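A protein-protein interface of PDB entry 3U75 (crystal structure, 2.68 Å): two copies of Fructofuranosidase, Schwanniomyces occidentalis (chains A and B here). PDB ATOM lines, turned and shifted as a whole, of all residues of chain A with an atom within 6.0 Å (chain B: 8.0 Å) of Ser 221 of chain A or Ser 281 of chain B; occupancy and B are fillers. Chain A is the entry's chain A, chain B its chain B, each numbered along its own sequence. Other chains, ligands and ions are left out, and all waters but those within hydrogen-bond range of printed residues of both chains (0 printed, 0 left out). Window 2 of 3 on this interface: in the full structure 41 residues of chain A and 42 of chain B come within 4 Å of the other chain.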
ATOM      1  N   GLU A 200     -16.217  34.193 -26.585  1.00  0.00           N
ATOM      2  CA  GLU A 200     -16.595  33.092 -27.457  1.00  0.00           C
ATOM      3  C   GLU A 200     -15.356  32.339 -27.909  1.00  0.00           C
ATOM      4  O   GLU A 200     -15.461  31.326 -28.604  1.00  0.00           O
ATOM      5  CB  GLU A 200     -17.369  33.602 -28.673  1.00  0.00           C
ATOM      6  CG  GLU A 200     -18.843  33.847 -28.411  1.00  0.00           C
ATOM      7  CD  GLU A 200     -19.689  33.953 -29.690  1.00  0.00           C
ATOM      8  OE1 GLU A 200     -19.303  33.412 -30.768  1.00  0.00           O
ATOM      9  OE2 GLU A 200     -20.771  34.584 -29.604  1.00  0.00           O
ATOM     10  N   TYR A 201     -14.189  32.844 -27.497  1.00  0.00           N
ATOM     11  CA  TYR A 201     -12.892  32.382 -27.981  1.00  0.00           C
ATOM     12  C   TYR A 201     -12.889  32.285 -29.488  1.00  0.00           C
ATOM     13  O   TYR A 201     -12.526  31.255 -30.053  1.00  0.00           O
ATOM     14  CB  TYR A 201     -12.497  31.016 -27.417  1.00  0.00           C
ATOM     15  CG  TYR A 201     -12.609  30.908 -25.948  1.00  0.00           C
ATOM     16  CD1 TYR A 201     -13.668  30.216 -25.378  1.00  0.00           C
ATOM     17  CD2 TYR A 201     -11.662  31.513 -25.101  1.00  0.00           C
ATOM     18  CE1 TYR A 201     -13.787  30.100 -23.997  1.00  0.00           C
ATOM     19  CE2 TYR A 201     -11.777  31.412 -23.705  1.00  0.00           C
ATOM     20  CZ  TYR A 201     -12.845  30.697 -23.171  1.00  0.00           C
ATOM     21  OH  TYR A 201     -12.985  30.579 -21.817  1.00  0.00           O
ATOM     22  N   LYS A 202     -13.311  33.346 -30.141  1.00  0.00           N
ATOM     23  CA  LYS A 202     -13.102  33.443 -31.546  1.00  0.00           C
ATOM     24  C   LYS A 202     -12.327  34.724 -31.777  1.00  0.00           C
ATOM     25  O   LYS A 202     -12.616  35.770 -31.150  1.00  0.00           O
ATOM     26  CB  LYS A 202     -14.442  33.491 -32.293  1.00  0.00           C
ATOM     27  CG  LYS A 202     -15.124  32.167 -32.455  1.00  0.00           C
ATOM     28  CD  LYS A 202     -16.429  32.364 -33.172  1.00  0.00           C
ATOM     29  CE  LYS A 202     -17.272  31.089 -33.186  1.00  0.00           C
ATOM     30  NZ  LYS A 202     -17.922  30.928 -31.882  1.00  0.00           N
ATOM     31  N   ILE A 203     -11.329  34.622 -32.649  1.00  0.00           N
ATOM     32  CA  ILE A 203     -10.848  35.758 -33.408  1.00  0.00           C
ATOM     33  C   ILE A 203     -11.720  35.796 -34.680  1.00  0.00           C
ATOM     34  O   ILE A 203     -11.925  34.769 -35.343  1.00  0.00           O
ATOM     35  CB  ILE A 203      -9.345  35.607 -33.762  1.00  0.00           C
ATOM     36  CG1 ILE A 203      -8.478  35.742 -32.511  1.00  0.00           C
ATOM     37  CG2 ILE A 203      -8.927  36.657 -34.758  1.00  0.00           C
ATOM     38  CD1 ILE A 203      -7.036  35.331 -32.714  1.00  0.00           C
ATOM     39  N   ASN A 219     -14.022  32.556 -38.613  1.00  0.00           N
ATOM     40  CA  ASN A 219     -13.675  32.518 -37.209  1.00  0.00           C
ATOM     41  C   ASN A 219     -12.442  31.639 -36.986  1.00  0.00           C
ATOM     42  O   ASN A 219     -12.221  30.681 -37.742  1.00  0.00           O
ATOM     43  CB  ASN A 219     -14.844  31.947 -36.427  1.00  0.00           C
ATOM     44  CG  ASN A 219     -16.123  32.771 -36.590  1.00  0.00           C
ATOM     45  OD1 ASN A 219     -16.063  33.990 -36.747  1.00  0.00           O
ATOM     46  ND2 ASN A 219     -17.290  32.087 -36.541  1.00  0.00           N
ATOM     47  N   PHE A 220     -11.641  31.963 -35.962  1.00  0.00           N
ATOM     48  CA  PHE A 220     -10.422  31.205 -35.629  1.00  0.00           C
ATOM     49  C   PHE A 220     -10.327  30.997 -34.109  1.00  0.00           C
ATOM     50  O   PHE A 220     -10.371  31.966 -33.331  1.00  0.00           O
ATOM     51  CB  PHE A 220      -9.175  31.926 -36.185  1.00  0.00           C
ATOM     52  CG  PHE A 220      -7.830  31.298 -35.785  1.00  0.00           C
ATOM     53  CD1 PHE A 220      -7.237  30.326 -36.570  1.00  0.00           C
ATOM     54  CD2 PHE A 220      -7.137  31.733 -34.651  1.00  0.00           C
ATOM     55  CE1 PHE A 220      -5.994  29.753 -36.234  1.00  0.00           C
ATOM     56  CE2 PHE A 220      -5.885  31.155 -34.293  1.00  0.00           C
ATOM     57  CZ  PHE A 220      -5.324  30.153 -35.100  1.00  0.00           C
ATOM     58  N   SER A 221     -10.211  29.728 -33.702  1.00  0.00           N
ATOM     59  CA  SER A 221     -10.055  29.352 -32.293  1.00  0.00           C
ATOM     60  C   SER A 221      -8.924  28.369 -32.180  1.00  0.00           C
ATOM     61  O   SER A 221      -8.948  27.327 -32.807  1.00  0.00           O
ATOM     62  CB  SER A 221     -11.337  28.711 -31.725  1.00  0.00           C
ATOM     63  OG  SER A 221     -12.486  29.564 -31.820  1.00  0.00           O
ATOM     64  N   SER A 222      -7.918  28.705 -31.387  1.00  0.00           N
ATOM     65  CA  SER A 222      -6.817  27.777 -31.114  1.00  0.00           C
ATOM     66  C   SER A 222      -5.916  28.277 -29.975  1.00  0.00           C
ATOM     67  O   SER A 222      -6.210  29.299 -29.361  1.00  0.00           O
ATOM     68  CB  SER A 222      -6.008  27.492 -32.379  1.00  0.00           C
ATOM     69  OG  SER A 222      -5.286  26.274 -32.241  1.00  0.00           O
ATOM     70  N   GLY A 223      -4.847  27.525 -29.701  1.00  0.00           N
ATOM     71  CA  GLY A 223      -3.900  27.812 -28.622  1.00  0.00           C
ATOM     72  C   GLY A 223      -4.486  27.689 -27.234  1.00  0.00           C
ATOM     73  O   GLY A 223      -5.425  26.941 -27.019  1.00  0.00           O
ATOM     74  N   TYR A 225      -6.679  28.826 -24.243  1.00  0.00           N
ATOM     75  CA  TYR A 225      -7.892  29.643 -24.211  1.00  0.00           C
ATOM     76  C   TYR A 225      -7.898  30.665 -23.090  1.00  0.00           C
ATOM     77  O   TYR A 225      -8.203  31.822 -23.337  1.00  0.00           O
ATOM     78  CB  TYR A 225      -9.172  28.791 -24.192  1.00  0.00           C
ATOM     79  CG  TYR A 225      -9.586  28.242 -25.553  1.00  0.00           C
ATOM     80  CD1 TYR A 225      -8.666  28.086 -26.581  1.00  0.00           C
ATOM     81  CD2 TYR A 225     -10.884  27.855 -25.793  1.00  0.00           C
ATOM     82  CE1 TYR A 225      -9.034  27.581 -27.786  1.00  0.00           C
ATOM     83  CE2 TYR A 225     -11.254  27.351 -27.016  1.00  0.00           C
ATOM     84  CZ  TYR A 225     -10.319  27.213 -27.994  1.00  0.00           C
ATOM     85  OH  TYR A 225     -10.680  26.688 -29.200  1.00  0.00           O
ATOM     86  N   TYR A 229     -10.011  35.701 -25.121  1.00  0.00           N
ATOM     87  CA  TYR A 229      -9.215  36.160 -26.243  1.00  0.00           C
ATOM     88  C   TYR A 229      -9.256  37.685 -26.195  1.00  0.00           C
ATOM     89  O   TYR A 229     -10.241  38.238 -25.709  1.00  0.00           O
ATOM     90  CB  TYR A 229      -9.883  35.688 -27.511  1.00  0.00           C
ATOM     91  CG  TYR A 229      -9.525  34.293 -28.011  1.00  0.00           C
ATOM     92  CD1 TYR A 229      -8.872  33.353 -27.202  1.00  0.00           C
ATOM     93  CD2 TYR A 229      -9.886  33.918 -29.308  1.00  0.00           C
ATOM     94  CE1 TYR A 229      -8.578  32.095 -27.684  1.00  0.00           C
ATOM     95  CE2 TYR A 229      -9.588  32.687 -29.806  1.00  0.00           C
ATOM     96  CZ  TYR A 229      -8.942  31.764 -29.007  1.00  0.00           C
ATOM     97  OH  TYR A 229      -8.670  30.529 -29.586  1.00  0.00           O
ATOM     98  N   SER A 281      -0.552  22.895 -35.321  1.00  0.00           N
ATOM     99  CA  SER A 281      -1.474  23.333 -34.271  1.00  0.00           C
ATOM    100  C   SER A 281      -0.822  23.465 -32.857  1.00  0.00           C
ATOM    101  O   SER A 281      -1.410  23.022 -31.845  1.00  0.00           O
ATOM    102  CB  SER A 281      -2.619  22.350 -34.201  1.00  0.00           C
ATOM    103  OG  SER A 281      -2.095  21.066 -33.915  1.00  0.00           O
ATOM    104  N   THR A 283       0.965  25.486 -29.443  1.00  0.00           N
ATOM    105  CA  THR A 283       0.831  26.693 -28.603  1.00  0.00           C
ATOM    106  C   THR A 283       2.224  27.203 -28.335  1.00  0.00           C
ATOM    107  O   THR A 283       3.098  26.441 -27.898  1.00  0.00           O
ATOM    108  CB  THR A 283       0.057  26.387 -27.282  1.00  0.00           C
ATOM    109  OG1 THR A 283      -1.321  26.138 -27.584  1.00  0.00           O
ATOM    110  CG2 THR A 283       0.134  27.519 -26.283  1.00  0.00           C
ATOM    111  N   PHE B 220       0.608  11.846 -34.410  1.00  0.00           N
ATOM    112  CA  PHE B 220      -0.181  12.935 -33.838  1.00  0.00           C
ATOM    113  C   PHE B 220       0.737  13.977 -33.220  1.00  0.00           C
ATOM    114  O   PHE B 220       1.519  13.647 -32.311  1.00  0.00           O
ATOM    115  CB  PHE B 220      -1.165  12.372 -32.807  1.00  0.00           C
ATOM    116  CG  PHE B 220      -1.951  13.414 -32.052  1.00  0.00           C
ATOM    117  CD1 PHE B 220      -3.148  13.922 -32.568  1.00  0.00           C
ATOM    118  CD2 PHE B 220      -1.516  13.852 -30.786  1.00  0.00           C
ATOM    119  CE1 PHE B 220      -3.900  14.882 -31.851  1.00  0.00           C
ATOM    120  CE2 PHE B 220      -2.254  14.826 -30.042  1.00  0.00           C
ATOM    121  CZ  PHE B 220      -3.451  15.341 -30.573  1.00  0.00           C
ATOM    122  N   SER B 222       0.560  17.954 -31.543  1.00  0.00           N
ATOM    123  CA  SER B 222      -0.285  19.049 -31.084  1.00  0.00           C
ATOM    124  C   SER B 222       0.084  19.526 -29.678  1.00  0.00           C
ATOM    125  O   SER B 222       1.045  19.031 -29.084  1.00  0.00           O
ATOM    126  CB  SER B 222      -1.777  18.698 -31.183  1.00  0.00           C
ATOM    127  OG  SER B 222      -2.576  19.868 -31.317  1.00  0.00           O
ATOM    128  N   GLY B 223      -0.664  20.530 -29.202  1.00  0.00           N
ATOM    129  CA  GLY B 223      -0.471  21.153 -27.908  1.00  0.00           C
ATOM    130  C   GLY B 223       0.851  21.862 -27.774  1.00  0.00           C
ATOM    131  O   GLY B 223       1.450  22.263 -28.773  1.00  0.00           O
ATOM    132  N   TYR B 224       1.311  21.998 -26.531  1.00  0.00           N
ATOM    133  CA  TYR B 224       2.602  22.603 -26.235  1.00  0.00           C
ATOM    134  C   TYR B 224       3.721  21.608 -26.524  1.00  0.00           C
ATOM    135  O   TYR B 224       3.699  20.489 -26.010  1.00  0.00           O
ATOM    136  CB  TYR B 224       2.637  23.039 -24.771  1.00  0.00           C
ATOM    137  CG  TYR B 224       3.467  24.275 -24.507  1.00  0.00           C
ATOM    138  CD1 TYR B 224       3.110  25.516 -25.056  1.00  0.00           C
ATOM    139  CD2 TYR B 224       4.600  24.222 -23.701  1.00  0.00           C
ATOM    140  CE1 TYR B 224       3.872  26.658 -24.821  1.00  0.00           C
ATOM    141  CE2 TYR B 224       5.367  25.371 -23.461  1.00  0.00           C
ATOM    142  CZ  TYR B 224       4.993  26.573 -24.022  1.00  0.00           C
ATOM    143  OH  TYR B 224       5.736  27.702 -23.805  1.00  0.00           O
ATOM    144  N   TYR B 266      -3.381  17.517 -22.094  1.00  0.00           N
ATOM    145  CA  TYR B 266      -4.350  16.627 -22.682  1.00  0.00           C
ATOM    146  C   TYR B 266      -5.086  17.223 -23.842  1.00  0.00           C
ATOM    147  O   TYR B 266      -5.037  18.440 -24.064  1.00  0.00           O
ATOM    148  CB  TYR B 266      -5.338  16.102 -21.621  1.00  0.00           C
ATOM    149  CG  TYR B 266      -6.300  17.120 -21.048  1.00  0.00           C
ATOM    150  CD1 TYR B 266      -7.596  17.239 -21.538  1.00  0.00           C
ATOM    151  CD2 TYR B 266      -5.929  17.936 -19.989  1.00  0.00           C
ATOM    152  CE1 TYR B 266      -8.490  18.161 -21.000  1.00  0.00           C
ATOM    153  CE2 TYR B 266      -6.814  18.864 -19.440  1.00  0.00           C
ATOM    154  CZ  TYR B 266      -8.086  18.978 -19.957  1.00  0.00           C
ATOM    155  OH  TYR B 266      -8.948  19.910 -19.416  1.00  0.00           O
ATOM    156  N   PHE B 267      -5.773  16.340 -24.568  1.00  0.00           N
ATOM    157  CA  PHE B 267      -6.637  16.698 -25.688  1.00  0.00           C
ATOM    158  C   PHE B 267      -7.887  15.800 -25.704  1.00  0.00           C
ATOM    159  O   PHE B 267      -7.794  14.582 -25.519  1.00  0.00           O
ATOM    160  CB  PHE B 267      -5.921  16.537 -27.021  1.00  0.00           C
ATOM    161  CG  PHE B 267      -4.479  17.012 -27.046  1.00  0.00           C
ATOM    162  CD1 PHE B 267      -4.168  18.327 -27.381  1.00  0.00           C
ATOM    163  CD2 PHE B 267      -3.431  16.119 -26.813  1.00  0.00           C
ATOM    164  CE1 PHE B 267      -2.836  18.754 -27.456  1.00  0.00           C
ATOM    165  CE2 PHE B 267      -2.104  16.525 -26.880  1.00  0.00           C
ATOM    166  CZ  PHE B 267      -1.794  17.849 -27.201  1.00  0.00           C
ATOM    167  N   VAL B 268      -9.047  16.392 -25.971  1.00  0.00           N
ATOM    168  CA  VAL B 268     -10.335  15.700 -25.880  1.00  0.00           C
ATOM    169  C   VAL B 268     -11.025  15.541 -27.252  1.00  0.00           C
ATOM    170  O   VAL B 268     -11.429  16.538 -27.849  1.00  0.00           O
ATOM    171  CB  VAL B 268     -11.272  16.480 -24.955  1.00  0.00           C
ATOM    172  CG1 VAL B 268     -12.500  15.676 -24.614  1.00  0.00           C
ATOM    173  CG2 VAL B 268     -10.546  16.840 -23.681  1.00  0.00           C
ATOM    174  N   PRO B 278      -8.786  15.391 -32.189  1.00  0.00           N
ATOM    175  CA  PRO B 278      -9.310  16.292 -31.163  1.00  0.00           C
ATOM    176  C   PRO B 278     -10.511  17.108 -31.651  1.00  0.00           C
ATOM    177  O   PRO B 278     -10.480  17.672 -32.774  1.00  0.00           O
ATOM    178  CB  PRO B 278      -8.126  17.211 -30.860  1.00  0.00           C
ATOM    179  CG  PRO B 278      -7.263  17.143 -32.064  1.00  0.00           C
ATOM    180  CD  PRO B 278      -7.432  15.781 -32.632  1.00  0.00           C
ATOM    181  N   ASP B 279     -11.557  17.148 -30.817  1.00  0.00           N
ATOM    182  CA  ASP B 279     -12.717  18.007 -31.055  1.00  0.00           C
ATOM    183  C   ASP B 279     -12.306  19.432 -31.419  1.00  0.00           C
ATOM    184  O   ASP B 279     -12.736  19.952 -32.453  1.00  0.00           O
ATOM    185  CB  ASP B 279     -13.673  18.001 -29.865  1.00  0.00           C
ATOM    186  CG  ASP B 279     -14.375  16.664 -29.693  1.00  0.00           C
ATOM    187  OD1 ASP B 279     -13.853  15.651 -30.197  1.00  0.00           O
ATOM    188  OD2 ASP B 279     -15.447  16.613 -29.068  1.00  0.00           O
ATOM    189  N   ASP B 280     -11.454  20.037 -30.593  1.00  0.00           N
ATOM    190  CA  ASP B 280     -10.847  21.310 -30.938  1.00  0.00           C
ATOM    191  C   ASP B 280      -9.333  21.186 -30.973  1.00  0.00           C
ATOM    192  O   ASP B 280      -8.804  20.113 -30.762  1.00  0.00           O
ATOM    193  CB  ASP B 280     -11.260  22.386 -29.934  1.00  0.00           C
ATOM    194  CG  ASP B 280     -10.876  22.029 -28.520  1.00  0.00           C
ATOM    195  OD1 ASP B 280     -11.747  22.188 -27.652  1.00  0.00           O
ATOM    196  OD2 ASP B 280      -9.729  21.589 -28.276  1.00  0.00           O
ATOM    197  N   SER B 281      -8.642  22.294 -31.216  1.00  0.00           N
ATOM    198  CA  SER B 281      -7.185  22.316 -31.150  1.00  0.00           C
ATOM    199  C   SER B 281      -6.608  23.146 -29.961  1.00  0.00           C
ATOM    200  O   SER B 281      -5.587  23.807 -30.097  1.00  0.00           O
ATOM    201  CB  SER B 281      -6.627  22.846 -32.475  1.00  0.00           C
ATOM    202  OG  SER B 281      -7.089  24.169 -32.719  1.00  0.00           O
ATOM    203  N   GLN B 282      -7.229  23.132 -28.798  1.00  0.00           N
ATOM    204  CA  GLN B 282      -6.662  23.948 -27.732  1.00  0.00           C
ATOM    205  C   GLN B 282      -5.657  23.168 -26.913  1.00  0.00           C
ATOM    206  O   GLN B 282      -5.657  21.940 -26.938  1.00  0.00           O
ATOM    207  CB  GLN B 282      -7.748  24.497 -26.813  1.00  0.00           C
ATOM    208  CG  GLN B 282      -8.327  23.488 -25.836  1.00  0.00           C
ATOM    209  CD  GLN B 282      -9.577  24.002 -25.152  1.00  0.00           C
ATOM    210  OE1 GLN B 282      -9.518  24.738 -24.149  1.00  0.00           O
ATOM    211  NE2 GLN B 282     -10.725  23.605 -25.679  1.00  0.00           N
ATOM    212  N   THR B 283      -4.810  23.895 -26.197  1.00  0.00           N
ATOM    213  CA  THR B 283      -3.870  23.332 -25.247  1.00  0.00           C
ATOM    214  C   THR B 283      -4.435  23.446 -23.848  1.00  0.00           C
ATOM    215  O   THR B 283      -4.865  24.507 -23.424  1.00  0.00           O
ATOM    216  CB  THR B 283      -2.552  24.070 -25.314  1.00  0.00           C
ATOM    217  OG1 THR B 283      -1.872  23.708 -26.516  1.00  0.00           O
ATOM    218  CG2 THR B 283      -1.648  23.742 -24.141  1.00  0.00           C
ATOM    219  N   ARG B 284      -4.453  22.332 -23.138  1.00  0.00           N
ATOM    220  CA  ARG B 284      -4.898  22.315 -21.748  1.00  0.00           C
ATOM    221  C   ARG B 284      -4.029  21.376 -20.912  1.00  0.00           C
ATOM    222  O   ARG B 284      -3.601  20.305 -21.379  1.00  0.00           O
ATOM    223  CB  ARG B 284      -6.366  21.932 -21.641  1.00  0.00           C
ATOM    224  CG  ARG B 284      -7.359  23.089 -21.751  1.00  0.00           C
ATOM    225  CD  ARG B 284      -8.813  22.565 -21.792  1.00  0.00           C
ATOM    226  NE  ARG B 284      -9.031  21.644 -22.912  1.00  0.00           N
ATOM    227  CZ  ARG B 284     -10.163  20.984 -23.137  1.00  0.00           C
ATOM    228  NH1 ARG B 284     -11.195  21.148 -22.326  1.00  0.00           N
ATOM    229  NH2 ARG B 284     -10.263  20.165 -24.184  1.00  0.00           N
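O of Tyr 201 of chain A sits at hydrogen-bond distance from OG of Ser 221 of chain A.
The side-chain hydroxyl (OH) of Tyr 229 of chain A is in hydrogen-bond range of the backbone NH (N) of Ser 222 of chain A, at 2.7 Å.
The side-chain amide nitrogen (NE2) of Gln 282 of chain B is in hydrogen-bond range of the side-chain carboxylate (OD1) of Asp 280 of chain B (2.6 Å).
OE1 of Gln 282 of chain B sits close to NE of Arg 284 of chain B (3.4 Å).
Hydrophobic or aromatic side chains of chain A that line the printed part of chain B: Tyr 225.
Of the 14 printed residues of chain B, 6 touch a printed residue of chain A.
Hydrophobic or aromatic side chains of chain B that line the printed part of chain A: Tyr 224.
Among the printed residues, 11 pairs touch across the chains.
Among the printed residues, no Asp or Glu carboxylate lies within 4 Å of a Lys or Arg side-chain nitrogen of the other chain.
Of chain B, only Ser 281 comes within 4 Å of Ser 221 of chain A.
Printed residues of chain B within 4 Å of Tyr 225 of chain A: Gln 282 (3.5 Å).
Printed residues of chain B within 4 Å of Thr 283 of chain A: Gly 223, Tyr 224 and Thr 283.
Of the printed residues of chain A, Ser 222 of chain B touches Ser 281.
Of chain A, only Ser 221, Ser 222 and Gly 223 come within 4 Å of Ser 281 of chain B.
The nearest printed residue of chain B that does not touch Tyr 225 of chain A is Asp 280 of chain B (4.4 Å).
OG of Ser 222 of chain A lies within hydrogen-bond range of OG of Ser 281 of chain B, 2.8 Å away.
The backbone NH of Thr 283 of chain B sits at hydrogen-bond distance from the backbone carbonyl oxygen of Gly 223 of chain A (3.2 Å).
The side-chain hydroxyl (OG) of Ser 281 of chain A is in hydrogen-bond range of the side-chain hydroxyl (OG) of Ser 222 of chain B (2.9 Å).
O of Gly 223 of chain B sits at hydrogen-bond distance from N of Thr 283 of chain A, 3.3 Å away.
OG1 of Thr 283 of chain A lies within hydrogen-bond range of OG1 of Thr 283 of chain B (2.7 Å).
Ser 281 of chain B touches Ser 221 of chain A.
N of Gly 223 of chain A touches O of Ser 281 of chain B (3.8 Å).
Gln 282 of chain B touches Gly 223 of chain A.
Tyr 225 of chain A touches Gln 282 of chain B.
O of Ser 281 of chain A touches N of Gly 223 of chain B, at 3.7 Å.
CD1 of Tyr 224 of chain B touches O of Thr 283 of chain A, 3.0 Å away.
Ser 222 of chain A touches Ser 281 of chain B, and with the chains exchanged Ser 281 of chain A touches Ser 222 of chain B.
Gly 223 of chain A touches Ser 281 of chain B, and with the chains exchanged Ser 281 of chain A touches Gly 223 of chain B.
Gly 223 of chain A touches Thr 283 of chain B, and with the chains exchanged Thr 283 of chain A touches Gly 223 of chain B.
Thr 283 of chain A touches its own counterpart, Thr 283 of chain B.
5 positions are printed for both chains.
Of the 11 pairs that touch across the chains among the printed residues, 7 have their exchanged pair printed and touching as well.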
